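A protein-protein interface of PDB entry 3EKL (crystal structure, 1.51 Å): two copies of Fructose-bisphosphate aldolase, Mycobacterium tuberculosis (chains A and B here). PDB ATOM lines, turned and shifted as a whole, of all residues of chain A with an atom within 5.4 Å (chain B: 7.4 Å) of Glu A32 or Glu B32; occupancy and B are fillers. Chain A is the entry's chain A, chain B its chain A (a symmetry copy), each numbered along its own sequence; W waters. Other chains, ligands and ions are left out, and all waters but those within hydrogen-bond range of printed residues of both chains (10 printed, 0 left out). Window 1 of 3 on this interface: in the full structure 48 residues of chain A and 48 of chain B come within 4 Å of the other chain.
The backbone NH of Ser A31 lies within hydrogen-bond range of the side-chain hydroxyl of Ser B31, 2.9 Å away. The side-chain carboxylate (OE1) of Glu A32 lies close to the side-chain carboxylate (OE1) of Glu B32 (2.5 Å). ND2 of Asn A35 sits at hydrogen-bond distance from O of Gly B60, 2.9 Å away. ND2 of Asn A35 sits close to N of Gly B62 (3.4 Å).
OG of Ser A30 sits close to N of Glu A32. The side-chain hydroxyl of Ser A31 lies within hydrogen-bond range of the side-chain carboxylate of Glu A32, 3.3 Å away. The backbone carbonyl oxygen (O) of Ser A31 lies within hydrogen-bond range of the side-chain amide nitrogen (ND2) of Asn A35 (3.3 Å). The side-chain hydroxyl (OG) of Ser B30 lies close to the backbone NH (N) of Glu B32 (3.4 Å). The side-chain hydroxyl (OG) of Ser B30 lies within hydrogen-bond range of the side-chain hydroxyl (OG1) of Thr B33 (2.8 Å). O of Ser B31 lies within hydrogen-bond range of ND2 of Asn B35 (3.3 Å).
Ser A30 touches Ser B31. Glu B32 touches Ser A30 (OE2 to CB, 3.3 Å). Ser A31 touches Ser B30. Ser B30 touches Glu A32 (CB to OE2, 3.3 Å). CZ of Phe A59 touches CG of Glu B32, 3.9 Å away. CG of Phe A59 touches CG of Arg B314 (3.6 Å). Leu B317 touches Phe A59 (CB to CZ, 3.7 Å). Phe A59 touches Lys B318. Pro B313 touches Phe A283 (CG to CD2, 3.7 Å). Phe B59 touches Leu A317.
Glu A32 touches just these residues of chain B: Ser B30 (3.3 Å), Glu B32 (2.5 Å) and Phe B59 (3.9 Å). Of chain A, only Ser A30, Glu A32 and Phe A59 come within 4 Å of Glu B32. Printed residues of chain B within 4 Å of Phe A59: Glu B32 (3.9 Å), Arg B314 (3.6 Å), Leu B317 (3.7 Å) and Lys B318 (3.9 Å). Printed residues of chain B within 4 Å of Ser A30: Ser B31 (3.3 Å) and Glu B32 (3.3 Å). Of the printed residues of chain A, Phe B59 touches Glu A32 (3.9 Å) and Leu A317 (3.7 Å). Of the printed residues of chain B, Phe A283 touches Pro B313. Printed residues of chain B within 4 Å of Leu A317: Phe B59. Thr A29 touches none of the printed residues of chain B. Cys B28 touches none of the printed residues of chain A. The nearest residue of chain B that does not touch Glu A32 is Ser B31 (4.2 Å). The nearest residue of chain A that does not touch Glu B32 is Ser A31 (4.2 Å).
Printed residues of chain B that touch a printed residue of chain A: Ser B30, Ser B31, Glu B32, Phe B59, Gly B60, Gly B62, Pro B313, Arg B314, Leu B317 and Lys B318. Hydrophobic or aromatic side chains of chain B within 4 Å of the printed part of chain A: Phe B59, Pro B313 and Leu B317.
Ser A30 touches Ser B31, and with the chains exchanged Ser A31 touches Ser B30. Ser A30 touches Glu B32, and with the chains exchanged Glu A32 touches Ser B30. Glu A32 touches its own counterpart, Glu B32. Phe A59 touches Leu B317, and with the chains exchanged Leu A317 touches Phe B59.
Water W1 lies within hydrogen-bond range of the side-chain hydroxyl of Ser A30 (2.6 Å), the side-chain carboxylate of Glu B32 (2.7 Å) and the side-chain carboxylate of Glu A32 (3.4 Å). Water W4 bridges the side-chain hydroxyl (OG) of Ser B31 (2.7 Å) and the backbone carbonyl oxygen (O) of Thr A29 (2.9 Å). Water W9 lies within hydrogen-bond range of the side-chain hydroxyl of Thr B29 and the side-chain carboxylate of Glu A32. Water W8 bridges OG1 of Thr A29 (2.7 Å) and OE2 of Glu B32 (3.4 Å). Water W5 bridges O of Phe B59 and ND2 of Asn A35. Water W6 bridges the backbone carbonyl oxygen of Phe A59 (2.8 Å) and the side-chain amide nitrogen of Asn B35 (3.0 Å).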
ATOM      1  N   THR A  29     -21.313  26.272 -17.784  1.00  0.00           N
ATOM      2  CA  THR A  29     -21.985  27.481 -18.272  1.00  0.00           C
ATOM      3  C   THR A  29     -22.472  27.342 -19.703  1.00  0.00           C
ATOM      4  O   THR A  29     -22.997  28.298 -20.268  1.00  0.00           O
ATOM      5  CB  THR A  29     -21.016  28.690 -18.261  1.00  0.00           C
ATOM      6  OG1 THR A  29     -19.800  28.329 -18.932  1.00  0.00           O
ATOM      7  CG2 THR A  29     -20.684  29.106 -16.835  1.00  0.00           C
ATOM      8  N   SER A  30     -22.283  26.168 -20.302  1.00  0.00           N
ATOM      9  CA  SER A  30     -22.446  26.036 -21.750  1.00  0.00           C
ATOM     10  C   SER A  30     -22.444  24.584 -22.161  1.00  0.00           C
ATOM     11  O   SER A  30     -22.068  23.706 -21.381  1.00  0.00           O
ATOM     12  CB  SER A  30     -21.278  26.704 -22.455  1.00  0.00           C
ATOM     13  OG  SER A  30     -20.082  25.986 -22.153  1.00  0.00           O
ATOM     14  N   SER A  31     -22.837  24.336 -23.410  1.00  0.00           N
ATOM     15  CA  SER A  31     -22.731  23.001 -23.996  1.00  0.00           C
ATOM     16  C   SER A  31     -21.285  22.504 -23.942  1.00  0.00           C
ATOM     17  O   SER A  31     -21.037  21.346 -23.586  1.00  0.00           O
ATOM     18  CB  SER A  31     -23.263  23.009 -25.434  1.00  0.00           C
ATOM     19  OG  SER A  31     -22.681  24.068 -26.184  1.00  0.00           O
ATOM     20  N   GLU A  32     -20.313  23.373 -24.253  1.00  0.00           N
ATOM     21  CA  GLU A  32     -18.912  22.912 -24.301  1.00  0.00           C
ATOM     22  C   GLU A  32     -18.396  22.509 -22.929  1.00  0.00           C
ATOM     23  O   GLU A  32     -17.685  21.507 -22.786  1.00  0.00           O
ATOM     24  CB  GLU A  32     -17.978  23.994 -24.868  1.00  0.00           C
ATOM     25  CG  GLU A  32     -18.243  24.360 -26.323  1.00  0.00           C
ATOM     26  CD  GLU A  32     -19.100  25.585 -26.486  1.00  0.00           C
ATOM     27  OE1 GLU A  32     -19.953  25.882 -25.616  1.00  0.00           O
ATOM     28  OE2 GLU A  32     -18.890  26.262 -27.522  1.00  0.00           O
ATOM     29  N   THR A  33     -18.723  23.309 -21.920  1.00  0.00           N
ATOM     30  CA  THR A  33     -18.231  23.028 -20.569  1.00  0.00           C
ATOM     31  C   THR A  33     -18.948  21.812 -19.964  1.00  0.00           C
ATOM     32  O   THR A  33     -18.300  20.986 -19.305  1.00  0.00           O
ATOM     33  CB  THR A  33     -18.292  24.264 -19.653  1.00  0.00           C
ATOM     34  OG1 THR A  33     -19.621  24.814 -19.657  1.00  0.00           O
ATOM     35  CG2 THR A  33     -17.285  25.325 -20.126  1.00  0.00           C
ATOM     36  N   VAL A  34     -20.262  21.675 -20.190  1.00  0.00           N
ATOM     37  CA  VAL A  34     -20.950  20.424 -19.793  1.00  0.00           C
ATOM     38  C   VAL A  34     -20.263  19.213 -20.447  1.00  0.00           C
ATOM     39  O   VAL A  34     -19.960  18.202 -19.784  1.00  0.00           O
ATOM     40  CB  VAL A  34     -22.457  20.465 -20.142  1.00  0.00           C
ATOM     41  CG1 VAL A  34     -23.081  19.063 -20.064  1.00  0.00           C
ATOM     42  CG2 VAL A  34     -23.175  21.460 -19.230  1.00  0.00           C
ATOM     43  N   ASN A  35     -20.002  19.307 -21.748  1.00  0.00           N
ATOM     44  CA  ASN A  35     -19.372  18.198 -22.468  1.00  0.00           C
ATOM     45  C   ASN A  35     -18.005  17.877 -21.878  1.00  0.00           C
ATOM     46  O   ASN A  35     -17.635  16.693 -21.725  1.00  0.00           O
ATOM     47  CB  ASN A  35     -19.281  18.510 -23.964  1.00  0.00           C
ATOM     48  CG  ASN A  35     -20.585  18.239 -24.686  1.00  0.00           C
ATOM     49  OD1 ASN A  35     -21.387  17.433 -24.235  1.00  0.00           O
ATOM     50  ND2 ASN A  35     -20.795  18.904 -25.820  1.00  0.00           N
ATOM     51  N   ALA A  36     -17.250  18.922 -21.533  1.00  0.00           N
ATOM     52  CA  ALA A  36     -15.906  18.736 -20.987  1.00  0.00           C
ATOM     53  C   ALA A  36     -15.973  18.050 -19.623  1.00  0.00           C
ATOM     54  O   ALA A  36     -15.185  17.144 -19.330  1.00  0.00           O
ATOM     55  CB  ALA A  36     -15.175  20.081 -20.881  1.00  0.00           C
ATOM     56  N   ALA A  37     -16.926  18.473 -18.796  1.00  0.00           N
ATOM     57  CA  ALA A  37     -17.055  17.902 -17.455  1.00  0.00           C
ATOM     58  C   ALA A  37     -17.442  16.426 -17.522  1.00  0.00           C
ATOM     59  O   ALA A  37     -16.789  15.576 -16.890  1.00  0.00           O
ATOM     60  CB  ALA A  37     -18.050  18.688 -16.642  1.00  0.00           C
ATOM     61  N   PHE A  59     -25.968  33.393 -17.880  1.00  0.00           N
ATOM     62  CA  PHE A  59     -25.121  33.351 -19.076  1.00  0.00           C
ATOM     63  C   PHE A  59     -25.664  32.316 -20.065  1.00  0.00           C
ATOM     64  O   PHE A  59     -25.737  32.568 -21.285  1.00  0.00           O
ATOM     65  CB  PHE A  59     -23.674  33.030 -18.698  1.00  0.00           C
ATOM     66  CG  PHE A  59     -22.791  32.766 -19.880  1.00  0.00           C
ATOM     67  CD1 PHE A  59     -22.199  33.821 -20.581  1.00  0.00           C
ATOM     68  CD2 PHE A  59     -22.551  31.461 -20.290  1.00  0.00           C
ATOM     69  CE1 PHE A  59     -21.380  33.556 -21.691  1.00  0.00           C
ATOM     70  CE2 PHE A  59     -21.739  31.191 -21.392  1.00  0.00           C
ATOM     71  CZ  PHE A  59     -21.149  32.230 -22.083  1.00  0.00           C
ATOM     72  N   PHE A 283      -9.938  25.504 -19.286  1.00  0.00           N
ATOM     73  CA  PHE A 283     -10.721  25.733 -20.513  1.00  0.00           C
ATOM     74  C   PHE A 283     -10.088  26.849 -21.351  1.00  0.00           C
ATOM     75  O   PHE A 283      -9.894  26.700 -22.561  1.00  0.00           O
ATOM     76  CB  PHE A 283     -12.158  26.092 -20.141  1.00  0.00           C
ATOM     77  CG  PHE A 283     -13.120  26.090 -21.304  1.00  0.00           C
ATOM     78  CD1 PHE A 283     -13.758  24.915 -21.694  1.00  0.00           C
ATOM     79  CD2 PHE A 283     -13.408  27.276 -21.988  1.00  0.00           C
ATOM     80  CE1 PHE A 283     -14.670  24.900 -22.761  1.00  0.00           C
ATOM     81  CE2 PHE A 283     -14.314  27.272 -23.060  1.00  0.00           C
ATOM     82  CZ  PHE A 283     -14.947  26.097 -23.435  1.00  0.00           C
ATOM     83  N   LEU A 317     -12.271  25.584 -29.468  1.00  0.00           N
ATOM     84  CA  LEU A 317     -13.164  25.058 -28.418  1.00  0.00           C
ATOM     85  C   LEU A 317     -12.995  23.552 -28.173  1.00  0.00           C
ATOM     86  O   LEU A 317     -13.223  23.092 -27.051  1.00  0.00           O
ATOM     87  CB  LEU A 317     -14.622  25.450 -28.654  1.00  0.00           C
ATOM     88  CG  LEU A 317     -14.839  26.965 -28.499  1.00  0.00           C
ATOM     89  CD1 LEU A 317     -16.180  27.376 -29.078  1.00  0.00           C
ATOM     90  CD2 LEU A 317     -14.722  27.436 -27.066  1.00  0.00           C
ATOM     91  N   GLU A 321     -12.215  22.197 -24.526  1.00  0.00           N
ATOM     92  CA  GLU A 321     -12.962  21.058 -23.976  1.00  0.00           C
ATOM     93  C   GLU A 321     -12.039  19.941 -23.468  1.00  0.00           C
ATOM     94  O   GLU A 321     -12.232  19.425 -22.365  1.00  0.00           O
ATOM     95  CB  GLU A 321     -13.930  20.489 -25.021  1.00  0.00           C
ATOM     96  CG  GLU A 321     -14.894  19.449 -24.453  1.00  0.00           C
ATOM     97  CD  GLU A 321     -15.549  18.573 -25.502  1.00  0.00           C
ATOM     98  OE1 GLU A 321     -15.579  17.336 -25.301  1.00  0.00           O
ATOM     99  OE2 GLU A 321     -16.062  19.115 -26.506  1.00  0.00           O
ATOM    100  N   CYS B  28     -24.895  26.888 -36.348  1.00  0.00           N
ATOM    101  CA  CYS B  28     -24.565  26.978 -34.920  1.00  0.00           C
ATOM    102  C   CYS B  28     -23.997  25.657 -34.442  1.00  0.00           C
ATOM    103  O   CYS B  28     -24.221  24.618 -35.071  1.00  0.00           O
ATOM    104  CB  CYS B  28     -25.793  27.349 -34.100  1.00  0.00           C
ATOM    105  SG  CYS B  28     -26.445  28.993 -34.481  1.00  0.00           S
ATOM    106  N   THR B  29     -23.266  25.709 -33.324  1.00  0.00           N
ATOM    107  CA  THR B  29     -22.494  24.555 -32.851  1.00  0.00           C
ATOM    108  C   THR B  29     -22.543  24.399 -31.341  1.00  0.00           C
ATOM    109  O   THR B  29     -21.890  23.514 -30.796  1.00  0.00           O
ATOM    110  CB  THR B  29     -20.997  24.707 -33.221  1.00  0.00           C
ATOM    111  OG1 THR B  29     -20.532  25.997 -32.795  1.00  0.00           O
ATOM    112  CG2 THR B  29     -20.795  24.587 -34.725  1.00  0.00           C
ATOM    113  N   SER B  30     -23.293  25.263 -30.661  1.00  0.00           N
ATOM    114  CA  SER B  30     -23.168  25.374 -29.207  1.00  0.00           C
ATOM    115  C   SER B  30     -24.285  26.211 -28.634  1.00  0.00           C
ATOM    116  O   SER B  30     -24.996  26.904 -29.365  1.00  0.00           O
ATOM    117  CB  SER B  30     -21.862  26.071 -28.863  1.00  0.00           C
ATOM    118  OG  SER B  30     -21.919  27.419 -29.330  1.00  0.00           O
ATOM    119  N   SER B  31     -24.417  26.169 -27.309  1.00  0.00           N
ATOM    120  CA  SER B  31     -25.345  27.049 -26.603  1.00  0.00           C
ATOM    121  C   SER B  31     -25.036  28.515 -26.912  1.00  0.00           C
ATOM    122  O   SER B  31     -25.953  29.305 -27.171  1.00  0.00           O
ATOM    123  CB  SER B  31     -25.294  26.777 -25.094  1.00  0.00           C
ATOM    124  OG  SER B  31     -23.951  26.780 -24.625  1.00  0.00           O
ATOM    125  N   GLU B  32     -23.750  28.893 -26.931  1.00  0.00           N
ATOM    126  CA  GLU B  32     -23.411  30.315 -27.136  1.00  0.00           C
ATOM    127  C   GLU B  32     -23.786  30.796 -28.529  1.00  0.00           C
ATOM    128  O   GLU B  32     -24.290  31.911 -28.702  1.00  0.00           O
ATOM    129  CB  GLU B  32     -21.911  30.577 -26.923  1.00  0.00           C
ATOM    130  CG  GLU B  32     -21.421  30.335 -25.501  1.00  0.00           C
ATOM    131  CD  GLU B  32     -20.801  28.978 -25.303  1.00  0.00           C
ATOM    132  OE1 GLU B  32     -21.178  28.002 -25.995  1.00  0.00           O
ATOM    133  OE2 GLU B  32     -19.903  28.913 -24.429  1.00  0.00           O
ATOM    134  N   THR B  33     -23.508  29.969 -29.530  1.00  0.00           N
ATOM    135  CA  THR B  33     -23.789  30.366 -30.912  1.00  0.00           C
ATOM    136  C   THR B  33     -25.299  30.353 -31.192  1.00  0.00           C
ATOM    137  O   THR B  33     -25.802  31.259 -31.872  1.00  0.00           O
ATOM    138  CB  THR B  33     -22.992  29.537 -31.936  1.00  0.00           C
ATOM    139  OG1 THR B  33     -23.209  28.133 -31.706  1.00  0.00           O
ATOM    140  CG2 THR B  33     -21.492  29.859 -31.827  1.00  0.00           C
ATOM    141  N   VAL B  34     -26.031  29.360 -30.669  1.00  0.00           N
ATOM    142  CA  VAL B  34     -27.509  29.416 -30.750  1.00  0.00           C
ATOM    143  C   VAL B  34     -28.025  30.721 -30.121  1.00  0.00           C
ATOM    144  O   VAL B  34     -28.858  31.439 -30.706  1.00  0.00           O
ATOM    145  CB  VAL B  34     -28.165  28.181 -30.086  1.00  0.00           C
ATOM    146  CG1 VAL B  34     -29.667  28.410 -29.854  1.00  0.00           C
ATOM    147  CG2 VAL B  34     -27.902  26.935 -30.932  1.00  0.00           C
ATOM    148  N   ASN B  35     -27.528  31.046 -28.930  1.00  0.00           N
ATOM    149  CA  ASN B  35     -27.973  32.256 -28.238  1.00  0.00           C
ATOM    150  C   ASN B  35     -27.675  33.497 -29.070  1.00  0.00           C
ATOM    151  O   ASN B  35     -28.507  34.425 -29.156  1.00  0.00           O
ATOM    152  CB  ASN B  35     -27.338  32.345 -26.847  1.00  0.00           C
ATOM    153  CG  ASN B  35     -28.068  31.493 -25.828  1.00  0.00           C
ATOM    154  OD1 ASN B  35     -29.246  31.206 -25.991  1.00  0.00           O
ATOM    155  ND2 ASN B  35     -27.372  31.097 -24.765  1.00  0.00           N
ATOM    156  N   ALA B  36     -26.497  33.519 -29.696  1.00  0.00           N
ATOM    157  CA  ALA B  36     -26.089  34.672 -30.498  1.00  0.00           C
ATOM    158  C   ALA B  36     -26.994  34.821 -31.720  1.00  0.00           C
ATOM    159  O   ALA B  36     -27.412  35.931 -32.067  1.00  0.00           O
ATOM    160  CB  ALA B  36     -24.621  34.541 -30.924  1.00  0.00           C
ATOM    161  N   ALA B  37     -27.307  33.699 -32.362  1.00  0.00           N
ATOM    162  CA  ALA B  37     -28.143  33.737 -33.563  1.00  0.00           C
ATOM    163  C   ALA B  37     -29.555  34.221 -33.234  1.00  0.00           C
ATOM    164  O   ALA B  37     -30.069  35.148 -33.886  1.00  0.00           O
ATOM    165  CB  ALA B  37     -28.174  32.386 -34.227  1.00  0.00           C
ATOM    166  N   ILE B  38     -30.178  33.643 -32.206  1.00  0.00           N
ATOM    167  CA  ILE B  38     -31.546  34.060 -31.854  1.00  0.00           C
ATOM    168  C   ILE B  38     -31.613  35.538 -31.416  1.00  0.00           C
ATOM    169  O   ILE B  38     -32.518  36.272 -31.823  1.00  0.00           O
ATOM    170  CB  ILE B  38     -32.185  33.144 -30.783  1.00  0.00           C
ATOM    171  CG1 ILE B  38     -32.217  31.706 -31.289  1.00  0.00           C
ATOM    172  CG2 ILE B  38     -33.614  33.617 -30.480  1.00  0.00           C
ATOM    173  CD1 ILE B  38     -32.696  30.693 -30.253  1.00  0.00           C
ATOM    174  N   PHE B  59     -19.682  17.997 -33.072  1.00  0.00           N
ATOM    175  CA  PHE B  59     -19.024  18.870 -32.095  1.00  0.00           C
ATOM    176  C   PHE B  59     -19.944  19.097 -30.893  1.00  0.00           C
ATOM    177  O   PHE B  59     -19.504  19.048 -29.727  1.00  0.00           O
ATOM    178  CB  PHE B  59     -18.638  20.203 -32.740  1.00  0.00           C
ATOM    179  CG  PHE B  59     -18.149  21.224 -31.758  1.00  0.00           C
ATOM    180  CD1 PHE B  59     -16.817  21.232 -31.338  1.00  0.00           C
ATOM    181  CD2 PHE B  59     -19.024  22.178 -31.256  1.00  0.00           C
ATOM    182  CE1 PHE B  59     -16.376  22.191 -30.411  1.00  0.00           C
ATOM    183  CE2 PHE B  59     -18.594  23.134 -30.335  1.00  0.00           C
ATOM    184  CZ  PHE B  59     -17.278  23.148 -29.921  1.00  0.00           C
ATOM    185  N   GLY B  60     -21.225  19.332 -31.179  1.00  0.00           N
ATOM    186  CA  GLY B  60     -22.214  19.575 -30.116  1.00  0.00           C
ATOM    187  C   GLY B  60     -22.367  18.400 -29.167  1.00  0.00           C
ATOM    188  O   GLY B  60     -22.739  18.585 -27.998  1.00  0.00           O
ATOM    189  N   GLY B  62     -19.979  16.505 -28.111  1.00  0.00           N
ATOM    190  CA  GLY B  62     -18.775  16.382 -27.292  1.00  0.00           C
ATOM    191  C   GLY B  62     -17.781  15.354 -27.804  1.00  0.00           C
ATOM    192  O   GLY B  62     -18.160  14.406 -28.482  1.00  0.00           O
ATOM    193  N   LEU B  75     -28.693  19.946 -28.911  1.00  0.00           N
ATOM    194  CA  LEU B  75     -28.749  21.362 -29.263  1.00  0.00           C
ATOM    195  C   LEU B  75     -30.167  21.809 -29.604  1.00  0.00           C
ATOM    196  O   LEU B  75     -30.567  22.928 -29.259  1.00  0.00           O
ATOM    197  CB  LEU B  75     -27.771  21.703 -30.398  1.00  0.00           C
ATOM    198  CG  LEU B  75     -26.276  21.634 -30.056  1.00  0.00           C
ATOM    199  CD1 LEU B  75     -25.465  21.779 -31.334  1.00  0.00           C
ATOM    200  CD2 LEU B  75     -25.879  22.675 -29.021  1.00  0.00           C
ATOM    201  N   PHE B  78     -32.035  22.280 -26.261  1.00  0.00           N
ATOM    202  CA  PHE B  78     -31.590  23.546 -25.710  1.00  0.00           C
ATOM    203  C   PHE B  78     -32.309  24.703 -26.413  1.00  0.00           C
ATOM    204  O   PHE B  78     -32.843  25.608 -25.758  1.00  0.00           O
ATOM    205  CB  PHE B  78     -30.076  23.666 -25.888  1.00  0.00           C
ATOM    206  CG  PHE B  78     -29.537  25.004 -25.486  1.00  0.00           C
ATOM    207  CD1 PHE B  78     -29.154  25.259 -24.166  1.00  0.00           C
ATOM    208  CD2 PHE B  78     -29.419  26.035 -26.428  1.00  0.00           C
ATOM    209  CE1 PHE B  78     -28.673  26.510 -23.795  1.00  0.00           C
ATOM    210  CE2 PHE B  78     -28.949  27.286 -26.059  1.00  0.00           C
ATOM    211  CZ  PHE B  78     -28.577  27.529 -24.745  1.00  0.00           C
ATOM    212  N   PHE B 283     -17.793  35.778 -34.277  1.00  0.00           N
ATOM    213  CA  PHE B 283     -17.731  35.151 -32.944  1.00  0.00           C
ATOM    214  C   PHE B 283     -16.295  35.176 -32.408  1.00  0.00           C
ATOM    215  O   PHE B 283     -16.055  35.565 -31.261  1.00  0.00           O
ATOM    216  CB  PHE B 283     -18.244  33.715 -33.032  1.00  0.00           C
ATOM    217  CG  PHE B 283     -18.479  33.056 -31.696  1.00  0.00           C
ATOM    218  CD1 PHE B 283     -19.696  33.207 -31.035  1.00  0.00           C
ATOM    219  CD2 PHE B 283     -17.488  32.259 -31.114  1.00  0.00           C
ATOM    220  CE1 PHE B 283     -19.938  32.586 -29.800  1.00  0.00           C
ATOM    221  CE2 PHE B 283     -17.716  31.637 -29.877  1.00  0.00           C
ATOM    222  CZ  PHE B 283     -18.934  31.789 -29.232  1.00  0.00           C
ATOM    223  N   PRO B 313     -14.485  31.913 -18.727  1.00  0.00           N
ATOM    224  CA  PRO B 313     -14.965  31.850 -20.120  1.00  0.00           C
ATOM    225  C   PRO B 313     -16.096  32.822 -20.453  1.00  0.00           C
ATOM    226  O   PRO B 313     -16.180  33.296 -21.585  1.00  0.00           O
ATOM    227  CB  PRO B 313     -15.413  30.391 -20.274  1.00  0.00           C
ATOM    228  CG  PRO B 313     -14.517  29.647 -19.311  1.00  0.00           C
ATOM    229  CD  PRO B 313     -14.440  30.571 -18.107  1.00  0.00           C
ATOM    230  N   ARG B 314     -16.949  33.127 -19.486  1.00  0.00           N
ATOM    231  CA  ARG B 314     -18.039  34.071 -19.753  1.00  0.00           C
ATOM    232  C   ARG B 314     -17.512  35.433 -20.187  1.00  0.00           C
ATOM    233  O   ARG B 314     -18.181  36.133 -20.948  1.00  0.00           O
ATOM    234  CB  ARG B 314     -18.931  34.232 -18.533  1.00  0.00           C
ATOM    235  CG  ARG B 314     -19.615  32.931 -18.119  1.00  0.00           C
ATOM    236  CD  ARG B 314     -20.406  33.119 -16.859  1.00  0.00           C
ATOM    237  NE  ARG B 314     -19.511  33.394 -15.739  1.00  0.00           N
ATOM    238  CZ  ARG B 314     -19.907  33.730 -14.516  1.00  0.00           C
ATOM    239  NH1 ARG B 314     -21.200  33.840 -14.232  1.00  0.00           N
ATOM    240  NH2 ARG B 314     -18.999  33.960 -13.576  1.00  0.00           N
ATOM    241  N   LEU B 317     -16.676  35.027 -23.918  1.00  0.00           N
ATOM    242  CA  LEU B 317     -17.798  34.441 -24.674  1.00  0.00           C
ATOM    243  C   LEU B 317     -19.019  35.365 -24.765  1.00  0.00           C
ATOM    244  O   LEU B 317     -19.766  35.288 -25.746  1.00  0.00           O
ATOM    245  CB  LEU B 317     -18.160  33.043 -24.173  1.00  0.00           C
ATOM    246  CG  LEU B 317     -17.043  32.025 -24.459  1.00  0.00           C
ATOM    247  CD1 LEU B 317     -17.255  30.757 -23.654  1.00  0.00           C
ATOM    248  CD2 LEU B 317     -16.907  31.695 -25.929  1.00  0.00           C
ATOM    249  N   LYS B 318     -19.238  36.211 -23.758  1.00  0.00           N
ATOM    250  CA  LYS B 318     -20.273  37.246 -23.878  1.00  0.00           C
ATOM    251  C   LYS B 318     -19.957  38.146 -25.070  1.00  0.00           C
ATOM    252  O   LYS B 318     -20.835  38.430 -25.884  1.00  0.00           O
ATOM    253  CB  LYS B 318     -20.378  38.093 -22.606  1.00  0.00           C
ATOM    254  CG  LYS B 318     -21.110  37.434 -21.458  1.00  0.00           C
ATOM    255  CD  LYS B 318     -21.114  38.357 -20.255  1.00  0.00           C
ATOM    256  CE  LYS B 318     -21.842  37.737 -19.084  1.00  0.00           C
ATOM    257  NZ  LYS B 318     -21.719  38.592 -17.874  1.00  0.00           N
ATOM    258  N   ALA B 320     -18.047  37.471 -27.670  1.00  0.00           N
ATOM    259  CA  ALA B 320     -18.216  36.648 -28.880  1.00  0.00           C
ATOM    260  C   ALA B 320     -19.691  36.597 -29.280  1.00  0.00           C
ATOM    261  O   ALA B 320     -20.037  36.827 -30.447  1.00  0.00           O
ATOM    262  CB  ALA B 320     -17.701  35.247 -28.626  1.00  0.00           C
ATOM    263  N   GLU B 321     -20.553  36.304 -28.303  1.00  0.00           N
ATOM    264  CA  GLU B 321     -22.002  36.232 -28.533  1.00  0.00           C
ATOM    265  C   GLU B 321     -22.574  37.542 -29.092  1.00  0.00           C
ATOM    266  O   GLU B 321     -23.345  37.526 -30.055  1.00  0.00           O
ATOM    267  CB  GLU B 321     -22.738  35.860 -27.240  1.00  0.00           C
ATOM    268  CG  GLU B 321     -24.219  35.550 -27.451  1.00  0.00           C
ATOM    269  CD  GLU B 321     -25.050  35.605 -26.186  1.00  0.00           C
ATOM    270  OE1 GLU B 321     -26.141  36.224 -26.223  1.00  0.00           O
ATOM    271  OE2 GLU B 321     -24.640  35.007 -25.167  1.00  0.00           O
ATOM    272  N   ALA B 322     -22.210  38.668 -28.485  1.00  0.00           N
ATOM    273  CA  ALA B 322     -22.720  39.970 -28.917  1.00  0.00           C
ATOM    274  C   ALA B 322     -22.245  40.305 -30.335  1.00  0.00           C
ATOM    275  O   ALA B 322     -23.004  40.861 -31.133  1.00  0.00           O
ATOM    276  CB  ALA B 322     -22.326  41.046 -27.927  1.00  0.00           C
ATOM    277  N   MET B 324     -21.296  38.118 -32.743  1.00  0.00           N
ATOM    278  CA  MET B 324     -21.991  37.266 -33.698  1.00  0.00           C
ATOM    279  C   MET B 324     -23.433  37.738 -33.900  1.00  0.00           C
ATOM    280  O   MET B 324     -23.924  37.750 -35.040  1.00  0.00           O
ATOM    281  CB  MET B 324     -21.907  35.793 -33.273  1.00  0.00           C
ATOM    282  CG  MET B 324     -22.721  34.858 -34.164  1.00  0.00           C
ATOM    283  SD  MET B 324     -22.387  33.141 -33.766  1.00  0.00           S
ATOM    284  CE  MET B 324     -23.726  32.341 -34.674  1.00  0.00           C
ATOM    285  N   SER B 325     -24.098  38.178 -32.832  1.00  0.00           N
ATOM    286  CA  SER B 325     -25.471  38.699 -32.965  1.00  0.00           C
ATOM    287  C   SER B 325     -25.504  39.888 -33.927  1.00  0.00           C
ATOM    288  O   SER B 325     -26.410  39.983 -34.771  1.00  0.00           O
ATOM    289  CB  SER B 325     -26.061  39.100 -31.613  1.00  0.00           C
ATOM    290  OG  SER B 325     -26.265  37.961 -30.788  1.00  0.00           O
HETATM  291  O   HOH W   1     -18.076  27.315 -23.231  1.00  0.00           O
HETATM  292  O   HOH W   2     -16.694  18.601 -29.168  1.00  0.00           O
HETATM  293  O   HOH W   3     -24.803  35.081 -22.389  1.00  0.00           O
HETATM  294  O   HOH W   4     -23.850  28.857 -22.964  1.00  0.00           O
HETATM  295  O   HOH W   5     -19.399  20.852 -27.555  1.00  0.00           O
HETATM  296  O   HOH W   6     -24.659  31.417 -23.629  1.00  0.00           O
HETATM  297  O   HOH W   7     -19.555  28.502 -28.889  1.00  0.00           O
HETATM  298  O   HOH W   8     -18.750  29.256 -21.235  1.00  0.00           O
HETATM  299  O   HOH W   9     -18.720  26.650 -30.909  1.00  0.00           O
HETATM  300  O   HOH W  10     -21.266  22.829 -28.066  1.00  0.00           O
